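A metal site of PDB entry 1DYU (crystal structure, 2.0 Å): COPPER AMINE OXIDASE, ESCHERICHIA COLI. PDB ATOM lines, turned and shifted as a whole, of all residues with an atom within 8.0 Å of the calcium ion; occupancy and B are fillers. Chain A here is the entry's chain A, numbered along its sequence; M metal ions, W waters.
The side-chain carboxylate of Glu 573 lies close to the backbone NH of Arg 642 (3.0 Å).
The backbone NH (N) of Glu 573 lies close to the side-chain amide nitrogen (ND2) of Asn 671 (3.5 Å).
The side-chain carboxylate (OE1) of Glu 672 lies close to the side-chain carboxylate (OD2) of Asp 670.
OE2 of Glu 672 is in salt-bridge range of NH1 of Arg 642.
ND1 of His 644 lies within hydrogen-bond range of OE1 of Glu 647 (3.1 Å).
Merely in contact with the calcium ion: His 644 (3.7 Å).
Five residues have an atom within 4 Å of the calcium ion: Glu 573, His 644, Tyr 667, Asp 670 and Glu 672.
The nearest printed residue that does not touch the calcium ion is Glu 647 (4.2 Å).
O of Tyr 667 binds the calcium ion.
The side-chain carboxylate (OE2) of Glu 573 binds the calcium ion, 2.5 Å away.
Water W1 binds the calcium ion.
OE1 of Glu 672 binds the calcium ion (2.7 Å).
Slightly farther from the calcium ion lies the side-chain carboxylate (OD2) of Asp 670 (2.9 Å).
Slightly farther from the calcium ion lies the side-chain carboxylate (OE1) of Glu 573 (3.1 Å).
Water W1 lies within hydrogen-bond range of OE2 of Glu 647 (2.8 Å), ND1 of His 644 (3.2 Å) and OD2 of Asp 670 (3.4 Å).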
ATOM      1  N   GLU A 573     -28.658  28.857  15.212  1.00  0.00           N
ATOM      2  CA  GLU A 573     -27.604  27.870  14.924  1.00  0.00           C
ATOM      3  C   GLU A 573     -27.391  27.550  13.459  1.00  0.00           C
ATOM      4  O   GLU A 573     -26.219  27.388  13.067  1.00  0.00           O
ATOM      5  CB  GLU A 573     -27.860  26.579  15.686  1.00  0.00           C
ATOM      6  CG  GLU A 573     -28.027  26.806  17.179  1.00  0.00           C
ATOM      7  CD  GLU A 573     -28.405  25.504  17.885  1.00  0.00           C
ATOM      8  OE1 GLU A 573     -29.383  24.891  17.454  1.00  0.00           O
ATOM      9  OE2 GLU A 573     -27.676  25.198  18.855  1.00  0.00           O
ATOM     10  N   VAL A 640     -21.746  27.559  15.691  1.00  0.00           N
ATOM     11  CA  VAL A 640     -22.033  28.129  16.989  1.00  0.00           C
ATOM     12  C   VAL A 640     -23.321  27.406  17.434  1.00  0.00           C
ATOM     13  O   VAL A 640     -24.308  27.352  16.678  1.00  0.00           O
ATOM     14  CB  VAL A 640     -22.133  29.651  17.070  1.00  0.00           C
ATOM     15  CG1 VAL A 640     -22.198  30.099  18.517  1.00  0.00           C
ATOM     16  CG2 VAL A 640     -20.988  30.362  16.344  1.00  0.00           C
ATOM     17  N   THR A 641     -23.317  26.836  18.636  1.00  0.00           N
ATOM     18  CA  THR A 641     -24.486  26.090  19.108  1.00  0.00           C
ATOM     19  C   THR A 641     -24.718  26.506  20.540  1.00  0.00           C
ATOM     20  O   THR A 641     -23.831  27.117  21.145  1.00  0.00           O
ATOM     21  CB  THR A 641     -24.264  24.550  19.042  1.00  0.00           C
ATOM     22  OG1 THR A 641     -23.141  24.189  19.884  1.00  0.00           O
ATOM     23  CG2 THR A 641     -23.968  24.154  17.614  1.00  0.00           C
ATOM     24  N   ARG A 642     -25.906  26.194  21.029  1.00  0.00           N
ATOM     25  CA  ARG A 642     -26.240  26.528  22.385  1.00  0.00           C
ATOM     26  C   ARG A 642     -25.501  25.541  23.292  1.00  0.00           C
ATOM     27  O   ARG A 642     -25.364  24.379  22.922  1.00  0.00           O
ATOM     28  CB  ARG A 642     -27.768  26.443  22.620  1.00  0.00           C
ATOM     29  CG  ARG A 642     -27.989  26.729  24.093  1.00  0.00           C
ATOM     30  CD  ARG A 642     -27.923  28.212  24.499  1.00  0.00           C
ATOM     31  NE  ARG A 642     -29.198  28.858  24.175  1.00  0.00           N
ATOM     32  CZ  ARG A 642     -30.341  28.574  23.548  1.00  0.00           C
ATOM     33  NH1 ARG A 642     -30.521  27.411  22.965  1.00  0.00           N
ATOM     34  NH2 ARG A 642     -31.266  29.520  23.476  1.00  0.00           N
ATOM     35  N   TYR A 643     -25.019  26.027  24.433  1.00  0.00           N
ATOM     36  CA  TYR A 643     -24.290  25.146  25.351  1.00  0.00           C
ATOM     37  C   TYR A 643     -25.194  23.996  25.875  1.00  0.00           C
ATOM     38  O   TYR A 643     -26.314  24.276  26.271  1.00  0.00           O
ATOM     39  CB  TYR A 643     -23.860  25.955  26.562  1.00  0.00           C
ATOM     40  CG  TYR A 643     -23.265  25.065  27.664  1.00  0.00           C
ATOM     41  CD1 TYR A 643     -22.024  24.433  27.522  1.00  0.00           C
ATOM     42  CD2 TYR A 643     -24.007  24.845  28.821  1.00  0.00           C
ATOM     43  CE1 TYR A 643     -21.552  23.607  28.531  1.00  0.00           C
ATOM     44  CE2 TYR A 643     -23.540  24.031  29.849  1.00  0.00           C
ATOM     45  CZ  TYR A 643     -22.293  23.416  29.676  1.00  0.00           C
ATOM     46  OH  TYR A 643     -21.846  22.624  30.690  1.00  0.00           O
ATOM     47  N   HIS A 644     -24.680  22.787  25.861  1.00  0.00           N
ATOM     48  CA  HIS A 644     -25.341  21.559  26.320  1.00  0.00           C
ATOM     49  C   HIS A 644     -24.156  20.709  26.817  1.00  0.00           C
ATOM     50  O   HIS A 644     -23.159  20.477  26.128  1.00  0.00           O
ATOM     51  CB  HIS A 644     -26.211  20.895  25.240  1.00  0.00           C
ATOM     52  CG  HIS A 644     -27.428  21.659  24.811  1.00  0.00           C
ATOM     53  ND1 HIS A 644     -27.963  21.631  23.523  1.00  0.00           N
ATOM     54  CD2 HIS A 644     -28.259  22.519  25.472  1.00  0.00           C
ATOM     55  CE1 HIS A 644     -29.037  22.411  23.417  1.00  0.00           C
ATOM     56  NE2 HIS A 644     -29.233  22.977  24.600  1.00  0.00           N
ATOM     57  N   GLU A 647     -22.822  17.730  24.498  1.00  0.00           N
ATOM     58  CA  GLU A 647     -22.561  17.885  23.046  1.00  0.00           C
ATOM     59  C   GLU A 647     -21.087  18.283  23.065  1.00  0.00           C
ATOM     60  O   GLU A 647     -20.740  19.405  23.363  1.00  0.00           O
ATOM     61  CB  GLU A 647     -23.467  18.991  22.499  1.00  0.00           C
ATOM     62  CG  GLU A 647     -24.944  18.616  22.676  1.00  0.00           C
ATOM     63  CD  GLU A 647     -25.836  19.633  21.945  1.00  0.00           C
ATOM     64  OE1 GLU A 647     -25.513  20.836  21.851  1.00  0.00           O
ATOM     65  OE2 GLU A 647     -26.886  19.196  21.455  1.00  0.00           O
ATOM     66  N   LEU A 664     -22.137  17.650  15.096  1.00  0.00           N
ATOM     67  CA  LEU A 664     -22.541  19.037  14.857  1.00  0.00           C
ATOM     68  C   LEU A 664     -23.799  19.098  13.999  1.00  0.00           C
ATOM     69  O   LEU A 664     -24.543  20.049  14.218  1.00  0.00           O
ATOM     70  CB  LEU A 664     -21.368  19.804  14.253  1.00  0.00           C
ATOM     71  CG  LEU A 664     -20.369  20.415  15.259  1.00  0.00           C
ATOM     72  CD1 LEU A 664     -19.164  21.050  14.563  1.00  0.00           C
ATOM     73  CD2 LEU A 664     -21.097  21.480  16.064  1.00  0.00           C
ATOM     74  N   GLN A 666     -26.365  17.116  14.213  1.00  0.00           N
ATOM     75  CA  GLN A 666     -27.397  16.875  15.205  1.00  0.00           C
ATOM     76  C   GLN A 666     -27.486  18.041  16.185  1.00  0.00           C
ATOM     77  O   GLN A 666     -28.611  18.444  16.490  1.00  0.00           O
ATOM     78  CB  GLN A 666     -27.144  15.567  15.990  1.00  0.00           C
ATOM     79  CG  GLN A 666     -28.062  15.276  17.171  1.00  0.00           C
ATOM     80  CD  GLN A 666     -27.667  14.051  17.982  1.00  0.00           C
ATOM     81  OE1 GLN A 666     -27.482  12.915  17.542  1.00  0.00           O
ATOM     82  NE2 GLN A 666     -27.475  14.321  19.270  1.00  0.00           N
ATOM     83  N   TYR A 667     -26.368  18.606  16.686  1.00  0.00           N
ATOM     84  CA  TYR A 667     -26.410  19.688  17.634  1.00  0.00           C
ATOM     85  C   TYR A 667     -27.068  20.971  17.117  1.00  0.00           C
ATOM     86  O   TYR A 667     -27.638  21.715  17.900  1.00  0.00           O
ATOM     87  CB  TYR A 667     -25.019  20.071  18.216  1.00  0.00           C
ATOM     88  CG  TYR A 667     -24.135  18.925  18.680  1.00  0.00           C
ATOM     89  CD1 TYR A 667     -24.661  17.751  19.215  1.00  0.00           C
ATOM     90  CD2 TYR A 667     -22.742  19.010  18.623  1.00  0.00           C
ATOM     91  CE1 TYR A 667     -23.876  16.705  19.645  1.00  0.00           C
ATOM     92  CE2 TYR A 667     -21.920  17.965  19.057  1.00  0.00           C
ATOM     93  CZ  TYR A 667     -22.498  16.808  19.568  1.00  0.00           C
ATOM     94  OH  TYR A 667     -21.711  15.754  20.004  1.00  0.00           O
ATOM     95  N   SER A 668     -27.006  21.254  15.854  1.00  0.00           N
ATOM     96  CA  SER A 668     -27.563  22.402  15.193  1.00  0.00           C
ATOM     97  C   SER A 668     -28.888  22.134  14.446  1.00  0.00           C
ATOM     98  O   SER A 668     -29.641  23.052  14.089  1.00  0.00           O
ATOM     99  CB  SER A 668     -26.503  22.902  14.201  1.00  0.00           C
ATOM    100  OG  SER A 668     -26.277  21.998  13.131  1.00  0.00           O
ATOM    101  N   LYS A 669     -29.235  20.880  14.210  1.00  0.00           N
ATOM    102  CA  LYS A 669     -30.433  20.422  13.534  1.00  0.00           C
ATOM    103  C   LYS A 669     -31.702  21.198  13.892  1.00  0.00           C
ATOM    104  O   LYS A 669     -32.501  21.573  13.067  1.00  0.00           O
ATOM    105  CB  LYS A 669     -30.832  18.979  13.941  1.00  0.00           C
ATOM    106  CG  LYS A 669     -31.439  18.268  12.744  1.00  0.00           C
ATOM    107  CD  LYS A 669     -31.451  16.745  12.848  1.00  0.00           C
ATOM    108  CE  LYS A 669     -32.536  16.153  11.955  1.00  0.00           C
ATOM    109  NZ  LYS A 669     -33.786  16.973  12.029  1.00  0.00           N
ATOM    110  N   ASP A 670     -31.924  21.460  15.154  1.00  0.00           N
ATOM    111  CA  ASP A 670     -33.035  22.159  15.750  1.00  0.00           C
ATOM    112  C   ASP A 670     -33.045  23.647  15.463  1.00  0.00           C
ATOM    113  O   ASP A 670     -34.031  24.347  15.706  1.00  0.00           O
ATOM    114  CB  ASP A 670     -32.974  21.957  17.274  1.00  0.00           C
ATOM    115  CG  ASP A 670     -31.547  22.019  17.813  1.00  0.00           C
ATOM    116  OD1 ASP A 670     -30.560  21.498  17.252  1.00  0.00           O
ATOM    117  OD2 ASP A 670     -31.263  22.626  18.883  1.00  0.00           O
ATOM    118  N   ASN A 671     -31.930  24.169  14.925  1.00  0.00           N
ATOM    119  CA  ASN A 671     -31.857  25.589  14.615  1.00  0.00           C
ATOM    120  C   ASN A 671     -32.301  26.491  15.751  1.00  0.00           C
ATOM    121  O   ASN A 671     -33.181  27.315  15.524  1.00  0.00           O
ATOM    122  CB  ASN A 671     -32.768  25.899  13.419  1.00  0.00           C
ATOM    123  CG  ASN A 671     -32.473  27.243  12.790  1.00  0.00           C
ATOM    124  OD1 ASN A 671     -33.158  27.744  11.865  1.00  0.00           O
ATOM    125  ND2 ASN A 671     -31.394  27.819  13.323  1.00  0.00           N
ATOM    126  N   GLU A 672     -31.725  26.367  16.951  1.00  0.00           N
ATOM    127  CA  GLU A 672     -32.145  27.194  18.059  1.00  0.00           C
ATOM    128  C   GLU A 672     -31.552  28.609  17.983  1.00  0.00           C
ATOM    129  O   GLU A 672     -30.629  28.940  17.232  1.00  0.00           O
ATOM    130  CB  GLU A 672     -31.769  26.507  19.394  1.00  0.00           C
ATOM    131  CG  GLU A 672     -32.356  25.133  19.652  1.00  0.00           C
ATOM    132  CD  GLU A 672     -31.892  24.457  20.931  1.00  0.00           C
ATOM    133  OE1 GLU A 672     -30.772  23.863  21.017  1.00  0.00           O
ATOM    134  OE2 GLU A 672     -32.675  24.533  21.902  1.00  0.00           O
ATOM    135  N   SER A 673     -32.110  29.441  18.833  1.00  0.00           N
ATOM    136  CA  SER A 673     -31.738  30.821  18.989  1.00  0.00           C
ATOM    137  C   SER A 673     -30.358  31.001  19.643  1.00  0.00           C
ATOM    138  O   SER A 673     -29.990  30.311  20.584  1.00  0.00           O
ATOM    139  CB  SER A 673     -32.697  31.513  19.996  1.00  0.00           C
ATOM    140  OG  SER A 673     -32.263  32.860  20.152  1.00  0.00           O
ATOM    141  N   LEU A 674     -29.604  31.969  19.133  1.00  0.00           N
ATOM    142  CA  LEU A 674     -28.263  32.280  19.651  1.00  0.00           C
ATOM    143  C   LEU A 674     -28.284  33.711  20.160  1.00  0.00           C
ATOM    144  O   LEU A 674     -27.275  34.350  20.382  1.00  0.00           O
ATOM    145  CB  LEU A 674     -27.199  32.086  18.597  1.00  0.00           C
ATOM    146  CG  LEU A 674     -26.957  30.632  18.146  1.00  0.00           C
ATOM    147  CD1 LEU A 674     -25.955  30.591  16.996  1.00  0.00           C
ATOM    148  CD2 LEU A 674     -26.420  29.854  19.341  1.00  0.00           C
HETATM  149 CA    CA M   1     -28.511  23.003  19.772  1.00  0.00          CA
HETATM  150  O   HOH W   1     -29.204  20.656  20.757  1.00  0.00           O
